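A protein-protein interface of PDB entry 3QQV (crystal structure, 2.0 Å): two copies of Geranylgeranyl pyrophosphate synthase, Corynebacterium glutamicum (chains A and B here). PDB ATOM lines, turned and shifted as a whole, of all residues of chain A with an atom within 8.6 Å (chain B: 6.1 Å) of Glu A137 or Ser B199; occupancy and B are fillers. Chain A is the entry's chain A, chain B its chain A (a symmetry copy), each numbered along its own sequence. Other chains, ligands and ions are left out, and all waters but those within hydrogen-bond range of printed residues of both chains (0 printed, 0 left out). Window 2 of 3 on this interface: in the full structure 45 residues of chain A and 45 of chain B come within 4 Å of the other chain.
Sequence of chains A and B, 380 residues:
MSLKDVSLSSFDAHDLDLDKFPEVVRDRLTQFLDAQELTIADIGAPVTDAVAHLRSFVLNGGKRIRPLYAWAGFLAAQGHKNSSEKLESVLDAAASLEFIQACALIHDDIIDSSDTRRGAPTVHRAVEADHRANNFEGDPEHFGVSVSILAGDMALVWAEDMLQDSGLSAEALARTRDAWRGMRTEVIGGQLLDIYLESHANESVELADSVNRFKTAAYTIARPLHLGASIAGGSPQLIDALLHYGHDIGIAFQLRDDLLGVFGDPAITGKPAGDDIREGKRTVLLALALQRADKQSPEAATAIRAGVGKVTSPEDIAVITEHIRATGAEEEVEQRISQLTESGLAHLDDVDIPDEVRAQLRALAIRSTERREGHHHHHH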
ATOM      1  N   PRO A  46      17.242  41.091  29.141  1.00  0.00           N
ATOM      2  CA  PRO A  46      17.283  40.293  27.902  1.00  0.00           C
ATOM      3  C   PRO A  46      16.748  40.983  26.627  1.00  0.00           C
ATOM      4  O   PRO A  46      17.146  40.614  25.518  1.00  0.00           O
ATOM      5  CB  PRO A  46      16.401  39.088  28.239  1.00  0.00           C
ATOM      6  CG  PRO A  46      16.489  38.952  29.700  1.00  0.00           C
ATOM      7  CD  PRO A  46      16.555  40.351  30.221  1.00  0.00           C
ATOM      8  N   VAL A 127      22.648  35.408  16.831  1.00  0.00           N
ATOM      9  CA  VAL A 127      21.876  35.101  18.044  1.00  0.00           C
ATOM     10  C   VAL A 127      22.059  33.621  18.447  1.00  0.00           C
ATOM     11  O   VAL A 127      22.152  33.302  19.637  1.00  0.00           O
ATOM     12  CB  VAL A 127      20.365  35.498  17.892  1.00  0.00           C
ATOM     13  CG1 VAL A 127      19.521  34.969  19.052  1.00  0.00           C
ATOM     14  CG2 VAL A 127      20.213  37.013  17.815  1.00  0.00           C
ATOM     15  N   ASP A 130      25.213  33.221  20.366  1.00  0.00           N
ATOM     16  CA  ASP A 130      25.101  33.730  21.736  1.00  0.00           C
ATOM     17  C   ASP A 130      24.560  32.665  22.685  1.00  0.00           C
ATOM     18  O   ASP A 130      24.832  32.698  23.888  1.00  0.00           O
ATOM     19  CB  ASP A 130      24.203  34.967  21.785  1.00  0.00           C
ATOM     20  CG  ASP A 130      24.988  36.252  21.933  1.00  0.00           C
ATOM     21  OD1 ASP A 130      25.564  36.473  23.020  1.00  0.00           O
ATOM     22  OD2 ASP A 130      25.020  37.045  20.970  1.00  0.00           O
ATOM     23  N   HIS A 131      23.796  31.725  22.129  1.00  0.00           N
ATOM     24  CA  HIS A 131      23.198  30.630  22.891  1.00  0.00           C
ATOM     25  C   HIS A 131      24.196  29.492  23.143  1.00  0.00           C
ATOM     26  O   HIS A 131      23.973  28.640  24.007  1.00  0.00           O
ATOM     27  CB  HIS A 131      21.941  30.113  22.179  1.00  0.00           C
ATOM     28  CG  HIS A 131      20.953  29.453  23.091  1.00  0.00           C
ATOM     29  ND1 HIS A 131      20.481  30.054  24.239  1.00  0.00           N
ATOM     30  CD2 HIS A 131      20.333  28.252  23.013  1.00  0.00           C
ATOM     31  CE1 HIS A 131      19.622  29.245  24.834  1.00  0.00           C
ATOM     32  NE2 HIS A 131      19.515  28.146  24.110  1.00  0.00           N
ATOM     33  N   ASN A 134      26.063  30.689  26.315  1.00  0.00           N
ATOM     34  CA  ASN A 134      25.212  30.552  27.503  1.00  0.00           C
ATOM     35  C   ASN A 134      25.036  29.104  27.970  1.00  0.00           C
ATOM     36  O   ASN A 134      24.836  28.862  29.166  1.00  0.00           O
ATOM     37  CB  ASN A 134      23.831  31.179  27.260  1.00  0.00           C
ATOM     38  CG  ASN A 134      23.870  32.702  27.202  1.00  0.00           C
ATOM     39  OD1 ASN A 134      22.930  33.329  26.711  1.00  0.00           O
ATOM     40  ND2 ASN A 134      24.947  33.301  27.706  1.00  0.00           N
ATOM     41  N   ASN A 135      25.113  28.165  27.018  1.00  0.00           N
ATOM     42  CA  ASN A 135      24.870  26.722  27.231  1.00  0.00           C
ATOM     43  C   ASN A 135      23.507  26.401  27.862  1.00  0.00           C
ATOM     44  O   ASN A 135      23.404  25.552  28.754  1.00  0.00           O
ATOM     45  CB  ASN A 135      26.026  26.054  28.005  1.00  0.00           C
ATOM     46  CG  ASN A 135      27.285  25.885  27.162  1.00  0.00           C
ATOM     47  OD1 ASN A 135      27.220  25.552  25.977  1.00  0.00           O
ATOM     48  ND2 ASN A 135      28.442  26.100  27.780  1.00  0.00           N
ATOM     49  N   PHE A 136      22.468  27.080  27.378  1.00  0.00           N
ATOM     50  CA  PHE A 136      21.136  27.019  27.984  1.00  0.00           C
ATOM     51  C   PHE A 136      20.150  26.096  27.243  1.00  0.00           C
ATOM     52  O   PHE A 136      20.507  25.468  26.242  1.00  0.00           O
ATOM     53  CB  PHE A 136      20.570  28.435  28.144  1.00  0.00           C
ATOM     54  N   GLU A 137      18.918  26.030  27.751  1.00  0.00           N
ATOM     55  CA  GLU A 137      17.878  25.096  27.285  1.00  0.00           C
ATOM     56  C   GLU A 137      17.305  25.444  25.902  1.00  0.00           C
ATOM     57  O   GLU A 137      17.055  26.613  25.596  1.00  0.00           O
ATOM     58  CB  GLU A 137      16.748  25.037  28.329  1.00  0.00           C
ATOM     59  CG  GLU A 137      15.634  24.014  28.071  1.00  0.00           C
ATOM     60  CD  GLU A 137      15.923  22.635  28.649  1.00  0.00           C
ATOM     61  OE1 GLU A 137      17.010  22.429  29.228  1.00  0.00           O
ATOM     62  OE2 GLU A 137      15.048  21.752  28.526  1.00  0.00           O
ATOM     63  N   GLY A 138      17.102  24.422  25.073  1.00  0.00           N
ATOM     64  CA  GLY A 138      16.434  24.589  23.784  1.00  0.00           C
ATOM     65  C   GLY A 138      17.374  24.675  22.596  1.00  0.00           C
ATOM     66  O   GLY A 138      18.562  24.969  22.752  1.00  0.00           O
ATOM     67  N   ASP A 139      16.821  24.415  21.410  1.00  0.00           N
ATOM     68  CA  ASP A 139      17.546  24.463  20.137  1.00  0.00           C
ATOM     69  C   ASP A 139      17.969  25.903  19.807  1.00  0.00           C
ATOM     70  O   ASP A 139      17.108  26.773  19.648  1.00  0.00           O
ATOM     71  CB  ASP A 139      16.667  23.874  19.018  1.00  0.00           C
ATOM     72  CG  ASP A 139      17.344  23.886  17.648  1.00  0.00           C
ATOM     73  OD1 ASP A 139      18.574  23.678  17.563  1.00  0.00           O
ATOM     74  OD2 ASP A 139      16.628  24.086  16.643  1.00  0.00           O
ATOM     75  N   PRO A 140      19.296  26.157  19.717  1.00  0.00           N
ATOM     76  CA  PRO A 140      19.823  27.505  19.467  1.00  0.00           C
ATOM     77  C   PRO A 140      19.494  28.050  18.077  1.00  0.00           C
ATOM     78  O   PRO A 140      19.400  29.268  17.910  1.00  0.00           O
ATOM     79  CB  PRO A 140      21.341  27.328  19.619  1.00  0.00           C
ATOM     80  CG  PRO A 140      21.513  26.053  20.379  1.00  0.00           C
ATOM     81  CD  PRO A 140      20.389  25.188  19.921  1.00  0.00           C
ATOM     82  N   PHE A 143      15.907  29.223  18.175  1.00  0.00           N
ATOM     83  CA  PHE A 143      15.939  30.396  19.054  1.00  0.00           C
ATOM     84  C   PHE A 143      16.475  31.641  18.338  1.00  0.00           C
ATOM     85  O   PHE A 143      15.979  32.746  18.557  1.00  0.00           O
ATOM     86  CB  PHE A 143      16.774  30.102  20.308  1.00  0.00           C
ATOM     87  CG  PHE A 143      16.926  31.282  21.245  1.00  0.00           C
ATOM     88  CD1 PHE A 143      15.835  31.769  21.966  1.00  0.00           C
ATOM     89  CD2 PHE A 143      18.169  31.890  21.423  1.00  0.00           C
ATOM     90  CE1 PHE A 143      15.974  32.855  22.842  1.00  0.00           C
ATOM     91  CE2 PHE A 143      18.324  32.980  22.298  1.00  0.00           C
ATOM     92  CZ  PHE A 143      17.224  33.457  23.013  1.00  0.00           C
ATOM     93  N   GLY A 144      17.490  31.446  17.496  1.00  0.00           N
ATOM     94  CA  GLY A 144      18.069  32.520  16.692  1.00  0.00           C
ATOM     95  C   GLY A 144      17.055  33.082  15.713  1.00  0.00           C
ATOM     96  O   GLY A 144      16.890  34.299  15.615  1.00  0.00           O
ATOM     97  N   SER A 146      13.794  32.720  16.067  1.00  0.00           N
ATOM     98  CA  SER A 146      12.758  33.297  16.934  1.00  0.00           C
ATOM     99  C   SER A 146      13.026  34.745  17.338  1.00  0.00           C
ATOM    100  O   SER A 146      12.172  35.608  17.131  1.00  0.00           O
ATOM    101  CB  SER A 146      12.536  32.431  18.188  1.00  0.00           C
ATOM    102  OG  SER A 146      11.800  31.259  17.870  1.00  0.00           O
ATOM    103  N   VAL A 147      14.199  35.003  17.911  1.00  0.00           N
ATOM    104  CA  VAL A 147      14.615  36.361  18.277  1.00  0.00           C
ATOM    105  C   VAL A 147      14.652  37.289  17.050  1.00  0.00           C
ATOM    106  O   VAL A 147      14.314  38.465  17.153  1.00  0.00           O
ATOM    107  CB  VAL A 147      15.975  36.361  19.015  1.00  0.00           C
ATOM    108  CG1 VAL A 147      16.503  37.778  19.258  1.00  0.00           C
ATOM    109  CG2 VAL A 147      15.857  35.624  20.341  1.00  0.00           C
ATOM    110  N   ASP B 194       9.784  36.857  26.830  1.00  0.00           N
ATOM    111  CA  ASP B 194       9.145  35.553  26.974  1.00  0.00           C
ATOM    112  C   ASP B 194      10.046  34.411  26.505  1.00  0.00           C
ATOM    113  O   ASP B 194      10.219  33.417  27.220  1.00  0.00           O
ATOM    114  CB  ASP B 194       7.816  35.516  26.208  1.00  0.00           C
ATOM    115  CG  ASP B 194       6.837  34.496  26.776  1.00  0.00           C
ATOM    116  OD1 ASP B 194       6.848  34.266  28.004  1.00  0.00           O
ATOM    117  OD2 ASP B 194       6.044  33.927  25.994  1.00  0.00           O
ATOM    118  N   ILE B 195      10.629  34.563  25.318  1.00  0.00           N
ATOM    119  CA  ILE B 195      11.451  33.497  24.741  1.00  0.00           C
ATOM    120  C   ILE B 195      12.857  33.410  25.339  1.00  0.00           C
ATOM    121  O   ILE B 195      13.489  32.357  25.288  1.00  0.00           O
ATOM    122  CB  ILE B 195      11.462  33.527  23.205  1.00  0.00           C
ATOM    123  CG1 ILE B 195      12.088  34.817  22.671  1.00  0.00           C
ATOM    124  CG2 ILE B 195      10.043  33.359  22.695  1.00  0.00           C
ATOM    125  CD1 ILE B 195      12.252  34.827  21.165  1.00  0.00           C
ATOM    126  N   TYR B 196      13.324  34.510  25.924  1.00  0.00           N
ATOM    127  CA  TYR B 196      14.557  34.514  26.707  1.00  0.00           C
ATOM    128  C   TYR B 196      14.372  33.833  28.065  1.00  0.00           C
ATOM    129  O   TYR B 196      15.337  33.336  28.653  1.00  0.00           O
ATOM    130  CB  TYR B 196      15.062  35.940  26.909  1.00  0.00           C
ATOM    131  CG  TYR B 196      16.071  36.411  25.878  1.00  0.00           C
ATOM    132  CD1 TYR B 196      15.659  37.051  24.705  1.00  0.00           C
ATOM    133  CD2 TYR B 196      17.444  36.239  26.087  1.00  0.00           C
ATOM    134  CE1 TYR B 196      16.586  37.494  23.761  1.00  0.00           C
ATOM    135  CE2 TYR B 196      18.379  36.680  25.147  1.00  0.00           C
ATOM    136  CZ  TYR B 196      17.941  37.306  23.990  1.00  0.00           C
ATOM    137  OH  TYR B 196      18.856  37.745  23.062  1.00  0.00           O
ATOM    138  N   LEU B 197      13.139  33.834  28.570  1.00  0.00           N
ATOM    139  CA  LEU B 197      12.808  33.062  29.764  1.00  0.00           C
ATOM    140  C   LEU B 197      12.688  31.577  29.424  1.00  0.00           C
ATOM    141  O   LEU B 197      13.114  30.726  30.204  1.00  0.00           O
ATOM    142  CB  LEU B 197      11.522  33.566  30.430  1.00  0.00           C
ATOM    143  CG  LEU B 197      11.469  34.950  31.089  1.00  0.00           C
ATOM    144  CD1 LEU B 197      10.333  34.995  32.103  1.00  0.00           C
ATOM    145  CD2 LEU B 197      12.787  35.349  31.741  1.00  0.00           C
ATOM    146  N   GLU B 198      12.115  31.278  28.259  1.00  0.00           N
ATOM    147  CA  GLU B 198      12.000  29.900  27.777  1.00  0.00           C
ATOM    148  C   GLU B 198      13.354  29.256  27.474  1.00  0.00           C
ATOM    149  O   GLU B 198      13.542  28.062  27.721  1.00  0.00           O
ATOM    150  CB  GLU B 198      11.092  29.826  26.549  1.00  0.00           C
ATOM    151  CG  GLU B 198       9.607  29.846  26.874  1.00  0.00           C
ATOM    152  CD  GLU B 198       8.722  29.739  25.642  1.00  0.00           C
ATOM    153  OE1 GLU B 198       9.167  29.171  24.622  1.00  0.00           O
ATOM    154  OE2 GLU B 198       7.572  30.222  25.698  1.00  0.00           O
ATOM    155  N   SER B 199      14.291  30.051  26.956  1.00  0.00           N
ATOM    156  CA  SER B 199      15.625  29.560  26.616  1.00  0.00           C
ATOM    157  C   SER B 199      16.492  29.358  27.857  1.00  0.00           C
ATOM    158  O   SER B 199      17.240  28.390  27.937  1.00  0.00           O
ATOM    159  CB  SER B 199      16.323  30.499  25.623  1.00  0.00           C
ATOM    160  OG  SER B 199      17.073  31.506  26.286  1.00  0.00           O
ATOM    161  N   HIS B 200      16.383  30.266  28.822  1.00  0.00           N
ATOM    162  CA  HIS B 200      17.153  30.165  30.064  1.00  0.00           C
ATOM    163  C   HIS B 200      16.477  29.290  31.126  1.00  0.00           C
ATOM    164  O   HIS B 200      16.965  29.210  32.258  1.00  0.00           O
ATOM    165  CB  HIS B 200      17.459  31.560  30.628  1.00  0.00           C
ATOM    166  CG  HIS B 200      18.637  32.223  29.982  1.00  0.00           C
ATOM    167  ND1 HIS B 200      18.614  32.681  28.680  1.00  0.00           N
ATOM    168  CD2 HIS B 200      19.875  32.498  30.456  1.00  0.00           C
ATOM    169  CE1 HIS B 200      19.787  33.209  28.381  1.00  0.00           C
ATOM    170  NE2 HIS B 200      20.571  33.111  29.440  1.00  0.00           N
ATOM    171  N   ALA B 201      15.372  28.638  30.742  1.00  0.00           N
ATOM    172  CA  ALA B 201      14.514  27.842  31.640  1.00  0.00           C
ATOM    173  C   ALA B 201      14.267  28.541  32.981  1.00  0.00           C
ATOM    174  O   ALA B 201      14.428  27.940  34.049  1.00  0.00           O
ATOM    175  CB  ALA B 201      15.091  26.433  31.840  1.00  0.00           C
ATOM    176  N   ASN B 202      13.887  29.817  32.903  1.00  0.00           N
ATOM    177  CA  ASN B 202      13.784  30.692  34.072  1.00  0.00           C
ATOM    178  C   ASN B 202      12.621  30.326  34.995  1.00  0.00           C
ATOM    179  O   ASN B 202      11.609  29.782  34.554  1.00  0.00           O
ATOM    180  CB  ASN B 202      13.713  32.159  33.628  1.00  0.00           C
ATOM    181  CG  ASN B 202      13.888  33.134  34.778  1.00  0.00           C
ATOM    182  OD1 ASN B 202      12.923  33.485  35.462  1.00  0.00           O
ATOM    183  ND2 ASN B 202      15.120  33.585  34.992  1.00  0.00           N
ATOM    184  N   ARG B 282       6.894  29.588  30.218  1.00  0.00           N
ATOM    185  CA  ARG B 282       7.334  29.930  31.570  1.00  0.00           C
ATOM    186  C   ARG B 282       6.350  30.879  32.260  1.00  0.00           C
ATOM    187  O   ARG B 282       6.631  32.065  32.473  1.00  0.00           O
ATOM    188  CB  ARG B 282       8.759  30.501  31.580  1.00  0.00           C
ATOM    189  CG  ARG B 282       9.768  29.813  30.649  1.00  0.00           C
ATOM    190  CD  ARG B 282       9.917  28.297  30.848  1.00  0.00           C
ATOM    191  NE  ARG B 282      10.527  27.936  32.125  1.00  0.00           N
ATOM    192  CZ  ARG B 282      10.909  26.702  32.456  1.00  0.00           C
ATOM    193  NH1 ARG B 282      11.447  26.478  33.645  1.00  0.00           N
ATOM    194  NH2 ARG B 282      10.757  25.688  31.607  1.00  0.00           N
ATOM    195  N   ARG B 305      10.107  19.521  35.704  1.00  0.00           N
ATOM    196  CA  ARG B 305      11.267  20.046  34.957  1.00  0.00           C
ATOM    197  C   ARG B 305      11.662  19.251  33.708  1.00  0.00           C
ATOM    198  O   ARG B 305      12.040  19.840  32.695  1.00  0.00           O
ATOM    199  CB  ARG B 305      12.484  20.198  35.869  1.00  0.00           C
ATOM    200  CG  ARG B 305      12.464  21.455  36.701  1.00  0.00           C
ATOM    201  CD  ARG B 305      13.716  21.607  37.526  1.00  0.00           C
ATOM    202  NE  ARG B 305      13.656  22.785  38.390  1.00  0.00           N
ATOM    203  CZ  ARG B 305      13.483  22.755  39.708  1.00  0.00           C
ATOM    204  NH1 ARG B 305      13.447  23.887  40.395  1.00  0.00           N
ATOM    205  NH2 ARG B 305      13.353  21.596  40.348  1.00  0.00           N
ATOM    206  N   VAL B 308       8.275  19.720  30.997  1.00  0.00           N
ATOM    207  CA  VAL B 308       7.928  20.986  30.321  1.00  0.00           C
ATOM    208  C   VAL B 308       8.790  21.307  29.095  1.00  0.00           C
ATOM    209  O   VAL B 308      10.017  21.387  29.178  1.00  0.00           O
ATOM    210  CB  VAL B 308       7.859  22.202  31.296  1.00  0.00           C
ATOM    211  CG1 VAL B 308       6.642  22.088  32.188  1.00  0.00           C
ATOM    212  CG2 VAL B 308       9.135  22.343  32.131  1.00  0.00           C
ATOM    213  N   LYS B 310       8.948  19.346  26.440  1.00  0.00           N
ATOM    214  CA  LYS B 310       9.464  18.088  25.893  1.00  0.00           C
ATOM    215  C   LYS B 310       8.394  17.028  25.612  1.00  0.00           C
ATOM    216  O   LYS B 310       8.360  16.464  24.517  1.00  0.00           O
ATOM    217  CB  LYS B 310      10.577  17.526  26.786  1.00  0.00           C
ATOM    218  CG  LYS B 310      11.972  18.021  26.404  1.00  0.00           C
ATOM    219  CD  LYS B 310      13.031  17.601  27.416  1.00  0.00           C
ATOM    220  CE  LYS B 310      13.439  18.749  28.330  1.00  0.00           C
ATOM    221  NZ  LYS B 310      12.357  19.182  29.253  1.00  0.00           N
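The backbone NH (N) of Glu A137 lies within hydrogen-bond range of the backbone carbonyl oxygen (O) of Ser B199 (2.9 Å).
OE2 of Glu A137 is in salt-bridge range of NZ of Lys B310, at 3.8 Å.
O of Val B308 lies within hydrogen-bond range of NZ of Lys B310.
A ring nitrogen (ND1) of His B200 is in hydrogen-bond range of the side-chain hydroxyl of Ser B199, at 3.1 Å.
OG of Ser B199 lies within hydrogen-bond range of O of Tyr B196, 3.5 Å away.
A ring nitrogen (NE2) of His A131 is in hydrogen-bond range of the backbone carbonyl oxygen (O) of Glu A137 (3.3 Å).
The backbone carbonyl oxygen (O) of Tyr B196 sits at hydrogen-bond distance from a ring nitrogen (ND1) of His B200 (3.3 Å).
The side-chain amide oxygen (OD1) of Asn A134 sits close to the backbone carbonyl oxygen (O) of Asp A130 (3.5 Å).
CG of Tyr B196 touches CB of Pro A46, at 3.6 Å.
CB of Ser B199 touches CE1 of His A131, 3.6 Å away.
His B200 touches Asn A134.
O of Ser B199 touches CB of Phe A136 (3.3 Å).
Ile B195 touches Phe A143.
Phe A143 touches Ser B199.
Ile B195 touches Ser A146 (CD1 to CB, 3.8 Å).
Val A147 touches Ile B195.
CG2 of Val A147 touches CE1 of Tyr B196, at 3.97 Å.
Of the printed residues of chain B, Asn A134 touches His B200.
Asn A135 touches none of the printed residues of chain B.
Of the printed residues of chain B, Phe A136 touches Ser B199 (3.3 Å).
Glu A137 touches just these residues of chain B: Ser B199 and Lys B310.
Printed residues of chain B within 4 Å of Ser A146: Ile B195 (3.8 Å).
Printed residues of chain B within 4 Å of Val A147: Ile B195 and Tyr B196.
Of chain A, only His A131, Phe A136, Glu A137 and Phe A143 come within 4 Å of Ser B199.
Printed residues of chain A within 4 Å of Lys B310: Glu A137 (3.4 Å).
The nearest residue of chain B that does not touch Glu A137 is Ala B201 (4.1 Å).
Of the 13 printed residues of chain B, 5 touch a printed residue of chain A.
Hydrophobic or aromatic side chains of chain B within 4 Å of the printed part of chain A: Ile B195, Tyr B196 and His B200.
Of the 15 printed residues of chain A, 8 touch a printed residue of chain B.
Hydrophobic or aromatic side chains of chain A that line the printed part of chain B: Pro A46, His A131, Phe A136, Phe A143 and Val A147.
Along chain A the printed residues that touch a printed residue of chain B span positions 46 to 147.
Among the printed residues, Asp or Glu carboxylates within 4 Å of a Lys or Arg side-chain nitrogen of the other chain: Glu A137 with Lys B310 (3.8 Å).
No position is printed for both chains.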
